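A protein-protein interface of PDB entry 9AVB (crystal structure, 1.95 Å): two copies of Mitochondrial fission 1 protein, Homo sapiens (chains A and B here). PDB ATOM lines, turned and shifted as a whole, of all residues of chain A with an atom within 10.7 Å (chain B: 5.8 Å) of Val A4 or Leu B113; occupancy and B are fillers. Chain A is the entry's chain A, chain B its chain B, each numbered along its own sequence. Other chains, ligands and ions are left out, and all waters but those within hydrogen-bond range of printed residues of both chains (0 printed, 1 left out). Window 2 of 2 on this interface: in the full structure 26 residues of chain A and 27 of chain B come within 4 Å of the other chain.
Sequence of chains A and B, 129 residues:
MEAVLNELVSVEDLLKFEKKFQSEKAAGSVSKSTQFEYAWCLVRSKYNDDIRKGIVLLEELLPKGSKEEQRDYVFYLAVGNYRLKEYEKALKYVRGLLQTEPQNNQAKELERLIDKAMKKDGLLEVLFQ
Printed residues of chain A that touch a printed residue of chain B: Glu A2, Val A4, Leu A5 and Leu A8. Of the 12 printed residues of chain B, 4 touch a printed residue of chain A. Printed residues of chain B that touch a printed residue of chain A: Tyr B82, Glu B109, Leu B110 and Leu B113. Hydrophobic or aromatic side chains of chain B that line the printed part of chain A: Tyr B82, Leu B110 and Leu B113. Among the printed residues, 7 pairs touch across the chains. Among the printed residues, no Asp or Glu carboxylate lies within 4 Å of a Lys or Arg side-chain nitrogen of the other chain.
OE2 of Glu A2 lies within hydrogen-bond range of OH of Tyr B82 (2.7 Å).
No position is printed for both chains.
Of the printed residues of chain B, Glu A2 touches Tyr B82 (2.7 Å). Val A4 touches one residue of chain B. Asn A6 touches none of the printed residues of chain B. Lys A46 touches none of the printed residues of chain B. Of the printed residues of chain A, Glu B109 touches Leu A8. Printed residues of chain A within 4 Å of Leu B110: Leu A5 (3.9 Å) and Leu A8 (3.8 Å). No residue of chain A comes within 4 Å of Ile B114. No residue of chain A comes within 4 Å of Asp B115. No residue of chain A comes within 4 Å of Lys B116. The nearest residue of chain B that does not touch Val A4 is Glu B109 (5.4 Å). The nearest residue of chain A that does not touch Leu B113 is Leu A5 (4.02 Å).
Among the printed residues, merely in contact across the chains: Leu A8 with Glu B109, Leu A8 with Leu B110, Leu A8 with Leu B113, Val A4 with Leu B113, Leu A5 with Leu B110 and Leu A5 with Tyr B82.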
ATOM      1  N   MET A   1      -8.971  20.661   4.236  1.00  0.00           N
ATOM      2  CA  MET A   1     -10.410  20.595   4.471  1.00  0.00           C
ATOM      3  C   MET A   1     -10.846  19.264   5.087  1.00  0.00           C
ATOM      4  O   MET A   1     -10.241  18.210   4.843  1.00  0.00           O
ATOM      5  CB  MET A   1     -11.172  20.838   3.161  1.00  0.00           C
ATOM      6  CG  MET A   1     -11.004  22.262   2.630  1.00  0.00           C
ATOM      7  SD  MET A   1     -11.853  22.624   1.082  1.00  0.00           S
ATOM      8  CE  MET A   1     -12.179  21.000   0.463  1.00  0.00           C
ATOM      9  N   GLU A   2     -11.910  19.336   5.885  1.00  0.00           N
ATOM     10  CA  GLU A   2     -12.557  18.147   6.427  1.00  0.00           C
ATOM     11  C   GLU A   2     -12.958  17.183   5.309  1.00  0.00           C
ATOM     12  O   GLU A   2     -13.111  17.564   4.146  1.00  0.00           O
ATOM     13  CB  GLU A   2     -13.795  18.541   7.227  1.00  0.00           C
ATOM     14  CG  GLU A   2     -14.629  19.600   6.539  1.00  0.00           C
ATOM     15  CD  GLU A   2     -16.118  19.477   6.842  1.00  0.00           C
ATOM     16  OE1 GLU A   2     -16.628  18.329   6.823  1.00  0.00           O
ATOM     17  OE2 GLU A   2     -16.777  20.523   7.054  1.00  0.00           O
ATOM     18  N   ALA A   3     -13.187  15.925   5.697  1.00  0.00           N
ATOM     19  CA  ALA A   3     -13.284  14.825   4.734  1.00  0.00           C
ATOM     20  C   ALA A   3     -14.495  14.961   3.814  1.00  0.00           C
ATOM     21  O   ALA A   3     -14.390  14.782   2.595  1.00  0.00           O
ATOM     22  CB  ALA A   3     -13.339  13.495   5.483  1.00  0.00           C
ATOM     23  N   VAL A   4     -15.665  15.242   4.382  1.00  0.00           N
ATOM     24  CA  VAL A   4     -16.871  15.331   3.563  1.00  0.00           C
ATOM     25  C   VAL A   4     -16.743  16.469   2.561  1.00  0.00           C
ATOM     26  O   VAL A   4     -17.052  16.312   1.373  1.00  0.00           O
ATOM     27  CB  VAL A   4     -18.114  15.503   4.456  1.00  0.00           C
ATOM     28  CG1 VAL A   4     -19.339  15.767   3.603  1.00  0.00           C
ATOM     29  CG2 VAL A   4     -18.310  14.268   5.309  1.00  0.00           C
ATOM     30  N   LEU A   5     -16.267  17.627   3.025  1.00  0.00           N
ATOM     31  CA  LEU A   5     -16.092  18.773   2.139  1.00  0.00           C
ATOM     32  C   LEU A   5     -15.101  18.460   1.031  1.00  0.00           C
ATOM     33  O   LEU A   5     -15.350  18.752  -0.146  1.00  0.00           O
ATOM     34  CB  LEU A   5     -15.610  19.984   2.931  1.00  0.00           C
ATOM     35  CG  LEU A   5     -15.587  21.280   2.133  1.00  0.00           C
ATOM     36  CD1 LEU A   5     -16.967  21.559   1.573  1.00  0.00           C
ATOM     37  CD2 LEU A   5     -15.095  22.440   2.985  1.00  0.00           C
ATOM     38  N   ASN A   6     -13.951  17.895   1.401  1.00  0.00           N
ATOM     39  CA  ASN A   6     -12.924  17.588   0.418  1.00  0.00           C
ATOM     40  C   ASN A   6     -13.468  16.679  -0.673  1.00  0.00           C
ATOM     41  O   ASN A   6     -13.146  16.848  -1.857  1.00  0.00           O
ATOM     42  CB  ASN A   6     -11.731  16.951   1.116  1.00  0.00           C
ATOM     43  CG  ASN A   6     -10.573  16.729   0.184  1.00  0.00           C
ATOM     44  OD1 ASN A   6      -9.881  17.673  -0.198  1.00  0.00           O
ATOM     45  ND2 ASN A   6     -10.333  15.470  -0.170  1.00  0.00           N
ATOM     46  N   GLU A   7     -14.335  15.739  -0.302  1.00  0.00           N
ATOM     47  CA  GLU A   7     -14.807  14.768  -1.279  1.00  0.00           C
ATOM     48  C   GLU A   7     -15.777  15.428  -2.257  1.00  0.00           C
ATOM     49  O   GLU A   7     -15.661  15.234  -3.471  1.00  0.00           O
ATOM     50  CB  GLU A   7     -15.421  13.576  -0.536  1.00  0.00           C
ATOM     51  CG  GLU A   7     -15.808  12.363  -1.361  1.00  0.00           C
ATOM     52  CD  GLU A   7     -17.088  12.514  -2.144  1.00  0.00           C
ATOM     53  OE1 GLU A   7     -17.929  13.370  -1.779  1.00  0.00           O
ATOM     54  OE2 GLU A   7     -17.260  11.737  -3.114  1.00  0.00           O
ATOM     55  N   LEU A   8     -16.697  16.276  -1.765  1.00  0.00           N
ATOM     56  CA  LEU A   8     -17.658  16.878  -2.686  1.00  0.00           C
ATOM     57  C   LEU A   8     -16.995  17.912  -3.592  1.00  0.00           C
ATOM     58  O   LEU A   8     -17.403  18.077  -4.750  1.00  0.00           O
ATOM     59  CB  LEU A   8     -18.837  17.497  -1.916  1.00  0.00           C
ATOM     60  CG  LEU A   8     -18.622  18.736  -1.025  1.00  0.00           C
ATOM     61  CD1 LEU A   8     -18.746  19.981  -1.844  1.00  0.00           C
ATOM     62  CD2 LEU A   8     -19.633  18.751   0.134  1.00  0.00           C
ATOM     63  N   VAL A   9     -15.984  18.630  -3.086  1.00  0.00           N
ATOM     64  CA  VAL A   9     -15.256  19.557  -3.946  1.00  0.00           C
ATOM     65  C   VAL A   9     -14.456  18.789  -5.004  1.00  0.00           C
ATOM     66  O   VAL A   9     -14.384  19.197  -6.174  1.00  0.00           O
ATOM     67  CB  VAL A   9     -14.376  20.475  -3.072  1.00  0.00           C
ATOM     68  CG1 VAL A   9     -13.397  21.272  -3.906  1.00  0.00           C
ATOM     69  CG2 VAL A   9     -15.281  21.410  -2.240  1.00  0.00           C
ATOM     70  N   SER A  10     -13.897  17.638  -4.634  1.00  0.00           N
ATOM     71  CA  SER A  10     -13.167  16.845  -5.625  1.00  0.00           C
ATOM     72  C   SER A  10     -14.082  16.402  -6.758  1.00  0.00           C
ATOM     73  O   SER A  10     -13.686  16.424  -7.931  1.00  0.00           O
ATOM     74  CB  SER A  10     -12.527  15.635  -4.961  1.00  0.00           C
ATOM     75  OG  SER A  10     -11.512  16.073  -4.079  1.00  0.00           O
ATOM     76  N   VAL A  11     -15.310  16.000  -6.423  1.00  0.00           N
ATOM     77  CA  VAL A  11     -16.261  15.595  -7.453  1.00  0.00           C
ATOM     78  C   VAL A  11     -16.612  16.779  -8.341  1.00  0.00           C
ATOM     79  O   VAL A  11     -16.617  16.663  -9.565  1.00  0.00           O
ATOM     80  CB  VAL A  11     -17.516  14.971  -6.812  1.00  0.00           C
ATOM     81  CG1 VAL A  11     -18.590  14.762  -7.871  1.00  0.00           C
ATOM     82  CG2 VAL A  11     -17.168  13.649  -6.127  1.00  0.00           C
ATOM     83  N   GLU A  12     -16.871  17.946  -7.741  1.00  0.00           N
ATOM     84  CA  GLU A  12     -17.233  19.127  -8.523  1.00  0.00           C
ATOM     85  C   GLU A  12     -16.124  19.483  -9.518  1.00  0.00           C
ATOM     86  O   GLU A  12     -16.388  19.722 -10.699  1.00  0.00           O
ATOM     87  CB  GLU A  12     -17.525  20.307  -7.576  1.00  0.00           C
ATOM     88  CG  GLU A  12     -18.039  21.580  -8.262  1.00  0.00           C
ATOM     89  CD  GLU A  12     -19.549  21.566  -8.549  1.00  0.00           C
ATOM     90  OE1 GLU A  12     -20.229  20.521  -8.345  1.00  0.00           O
ATOM     91  OE2 GLU A  12     -20.060  22.619  -8.992  1.00  0.00           O
ATOM     92  N   LYS A  46     -11.585   9.042  -6.543  1.00  0.00           N
ATOM     93  CA  LYS A  46     -11.716   7.778  -5.819  1.00  0.00           C
ATOM     94  C   LYS A  46     -11.708   6.552  -6.723  1.00  0.00           C
ATOM     95  O   LYS A  46     -11.622   5.436  -6.201  1.00  0.00           O
ATOM     96  CB  LYS A  46     -12.986   7.757  -4.973  1.00  0.00           C
ATOM     97  CG  LYS A  46     -14.262   7.880  -5.766  1.00  0.00           C
ATOM     98  CD  LYS A  46     -15.456   7.705  -4.849  1.00  0.00           C
ATOM     99  CE  LYS A  46     -15.716   9.016  -4.158  1.00  0.00           C
ATOM    100  NZ  LYS A  46     -16.301  10.034  -5.102  1.00  0.00           N
ATOM    101  N   TYR B  82     -18.419  29.147   3.696  1.00  0.00           N
ATOM    102  CA  TYR B  82     -18.685  28.101   4.682  1.00  0.00           C
ATOM    103  C   TYR B  82     -17.464  27.842   5.553  1.00  0.00           C
ATOM    104  O   TYR B  82     -17.583  27.682   6.773  1.00  0.00           O
ATOM    105  CB  TYR B  82     -19.115  26.803   3.976  1.00  0.00           C
ATOM    106  CG  TYR B  82     -19.054  25.559   4.846  1.00  0.00           C
ATOM    107  CD1 TYR B  82     -19.915  25.394   5.924  1.00  0.00           C
ATOM    108  CD2 TYR B  82     -18.124  24.556   4.594  1.00  0.00           C
ATOM    109  CE1 TYR B  82     -19.871  24.250   6.717  1.00  0.00           C
ATOM    110  CE2 TYR B  82     -18.062  23.415   5.384  1.00  0.00           C
ATOM    111  CZ  TYR B  82     -18.939  23.271   6.453  1.00  0.00           C
ATOM    112  OH  TYR B  82     -18.882  22.142   7.264  1.00  0.00           O
ATOM    113  N   LYS B 108     -25.660  20.207  -3.147  1.00  0.00           N
ATOM    114  CA  LYS B 108     -26.597  19.800  -2.113  1.00  0.00           C
ATOM    115  C   LYS B 108     -25.866  19.339  -0.855  1.00  0.00           C
ATOM    116  O   LYS B 108     -26.235  19.728   0.259  1.00  0.00           O
ATOM    117  CB  LYS B 108     -27.520  18.700  -2.637  1.00  0.00           C
ATOM    118  CG  LYS B 108     -28.476  18.180  -1.560  1.00  0.00           C
ATOM    119  CD  LYS B 108     -29.516  19.254  -1.195  1.00  0.00           C
ATOM    120  CE  LYS B 108     -30.396  18.791  -0.020  1.00  0.00           C
ATOM    121  NZ  LYS B 108     -31.389  19.829   0.382  1.00  0.00           N
ATOM    122  N   GLU B 109     -24.821  18.517  -1.000  1.00  0.00           N
ATOM    123  CA  GLU B 109     -24.104  18.093   0.207  1.00  0.00           C
ATOM    124  C   GLU B 109     -23.474  19.285   0.918  1.00  0.00           C
ATOM    125  O   GLU B 109     -23.380  19.300   2.161  1.00  0.00           O
ATOM    126  CB  GLU B 109     -23.041  17.054  -0.116  1.00  0.00           C
ATOM    127  CG  GLU B 109     -23.632  15.718  -0.594  1.00  0.00           C
ATOM    128  CD  GLU B 109     -22.589  14.800  -1.225  1.00  0.00           C
ATOM    129  OE1 GLU B 109     -21.787  15.291  -2.050  1.00  0.00           O
ATOM    130  OE2 GLU B 109     -22.594  13.584  -0.918  1.00  0.00           O
ATOM    131  N   LEU B 110     -23.065  20.297   0.152  1.00  0.00           N
ATOM    132  CA  LEU B 110     -22.523  21.503   0.768  1.00  0.00           C
ATOM    133  C   LEU B 110     -23.613  22.236   1.551  1.00  0.00           C
ATOM    134  O   LEU B 110     -23.398  22.640   2.701  1.00  0.00           O
ATOM    135  CB  LEU B 110     -21.904  22.399  -0.302  1.00  0.00           C
ATOM    136  CG  LEU B 110     -21.396  23.775   0.150  1.00  0.00           C
ATOM    137  CD1 LEU B 110     -20.295  23.585   1.191  1.00  0.00           C
ATOM    138  CD2 LEU B 110     -20.895  24.585  -1.052  1.00  0.00           C
ATOM    139  N   GLU B 111     -24.802  22.392   0.950  1.00  0.00           N
ATOM    140  CA  GLU B 111     -25.950  22.932   1.684  1.00  0.00           C
ATOM    141  C   GLU B 111     -26.219  22.151   2.969  1.00  0.00           C
ATOM    142  O   GLU B 111     -26.460  22.751   4.024  1.00  0.00           O
ATOM    143  CB  GLU B 111     -27.200  22.957   0.790  1.00  0.00           C
ATOM    144  CG  GLU B 111     -28.358  23.736   1.405  1.00  0.00           C
ATOM    145  CD  GLU B 111     -29.663  23.622   0.606  1.00  0.00           C
ATOM    146  OE1 GLU B 111     -30.076  22.490   0.279  1.00  0.00           O
ATOM    147  OE2 GLU B 111     -30.285  24.664   0.326  1.00  0.00           O
ATOM    148  N   ARG B 112     -26.163  20.812   2.910  1.00  0.00           N
ATOM    149  CA  ARG B 112     -26.377  20.023   4.123  1.00  0.00           C
ATOM    150  C   ARG B 112     -25.326  20.335   5.181  1.00  0.00           C
ATOM    151  O   ARG B 112     -25.645  20.412   6.373  1.00  0.00           O
ATOM    152  CB  ARG B 112     -26.374  18.516   3.834  1.00  0.00           C
ATOM    153  CG  ARG B 112     -27.513  17.996   2.923  1.00  0.00           C
ATOM    154  CD  ARG B 112     -27.351  16.473   2.712  1.00  0.00           C
ATOM    155  NE  ARG B 112     -28.256  15.941   1.698  1.00  0.00           N
ATOM    156  CZ  ARG B 112     -29.551  15.742   1.903  1.00  0.00           C
ATOM    157  NH1 ARG B 112     -30.112  16.014   3.071  1.00  0.00           N
ATOM    158  NH2 ARG B 112     -30.303  15.260   0.915  1.00  0.00           N
ATOM    159  N   LEU B 113     -24.065  20.490   4.772  1.00  0.00           N
ATOM    160  CA  LEU B 113     -23.013  20.812   5.736  1.00  0.00           C
ATOM    161  C   LEU B 113     -23.255  22.177   6.376  1.00  0.00           C
ATOM    162  O   LEU B 113     -23.090  22.340   7.592  1.00  0.00           O
ATOM    163  CB  LEU B 113     -21.639  20.784   5.050  1.00  0.00           C
ATOM    164  CG  LEU B 113     -20.978  19.463   4.676  1.00  0.00           C
ATOM    165  CD1 LEU B 113     -19.705  19.749   3.897  1.00  0.00           C
ATOM    166  CD2 LEU B 113     -20.677  18.630   5.910  1.00  0.00           C
ATOM    167  N   ILE B 114     -23.641  23.166   5.566  1.00  0.00           N
ATOM    168  CA  ILE B 114     -23.912  24.511   6.062  1.00  0.00           C
ATOM    169  C   ILE B 114     -25.075  24.491   7.050  1.00  0.00           C
ATOM    170  O   ILE B 114     -25.027  25.131   8.111  1.00  0.00           O
ATOM    171  CB  ILE B 114     -24.196  25.463   4.886  1.00  0.00           C
ATOM    172  CG1 ILE B 114     -22.978  25.615   3.980  1.00  0.00           C
ATOM    173  CG2 ILE B 114     -24.646  26.834   5.395  1.00  0.00           C
ATOM    174  CD1 ILE B 114     -23.321  26.195   2.599  1.00  0.00           C
ATOM    175  N   ASP B 115     -26.150  23.775   6.698  1.00  0.00           N
ATOM    176  CA  ASP B 115     -27.298  23.629   7.591  1.00  0.00           C
ATOM    177  C   ASP B 115     -26.899  22.965   8.895  1.00  0.00           C
ATOM    178  O   ASP B 115     -27.298  23.406   9.979  1.00  0.00           O
ATOM    179  CB  ASP B 115     -28.398  22.809   6.915  1.00  0.00           C
ATOM    180  CG  ASP B 115     -29.184  23.611   5.929  1.00  0.00           C
ATOM    181  OD1 ASP B 115     -29.851  23.000   5.062  1.00  0.00           O
ATOM    182  OD2 ASP B 115     -29.127  24.853   6.010  1.00  0.00           O
ATOM    183  N   LYS B 116     -26.124  21.887   8.807  1.00  0.00           N
ATOM    184  CA  LYS B 116     -25.687  21.200  10.014  1.00  0.00           C
ATOM    185  C   LYS B 116     -24.878  22.125  10.920  1.00  0.00           C
ATOM    186  O   LYS B 116     -24.985  22.049  12.150  1.00  0.00           O
ATOM    187  CB  LYS B 116     -24.876  19.965   9.634  1.00  0.00           C
ATOM    188  CG  LYS B 116     -24.242  19.234  10.802  1.00  0.00           C
ATOM    189  CD  LYS B 116     -23.469  18.018  10.305  1.00  0.00           C
ATOM    190  CE  LYS B 116     -22.914  17.205  11.463  1.00  0.00           C
ATOM    191  NZ  LYS B 116     -22.033  16.096  11.003  1.00  0.00           N
ATOM    192  N   ALA B 117     -24.074  23.018  10.332  1.00  0.00           N
ATOM    193  CA  ALA B 117     -23.230  23.896  11.145  1.00  0.00           C
ATOM    194  C   ALA B 117     -24.028  25.033  11.768  1.00  0.00           C
ATOM    195  O   ALA B 117     -23.688  25.504  12.857  1.00  0.00           O
ATOM    196  CB  ALA B 117     -22.085  24.459  10.310  1.00  0.00           C
ATOM    197  N   MET B 118     -25.082  25.479  11.093  1.00  0.00           N
ATOM    198  CA  MET B 118     -25.974  26.496  11.634  1.00  0.00           C
ATOM    199  C   MET B 118     -26.865  25.937  12.735  1.00  0.00           C
ATOM    200  O   MET B 118     -27.295  26.681  13.625  1.00  0.00           O
ATOM    201  CB  MET B 118     -26.830  27.066  10.511  1.00  0.00           C
ATOM    202  CG  MET B 118     -26.139  28.132   9.690  1.00  0.00           C
ATOM    203  SD  MET B 118     -27.077  28.600   8.229  1.00  0.00           S
ATOM    204  CE  MET B 118     -28.243  27.231   8.140  1.00  0.00           C
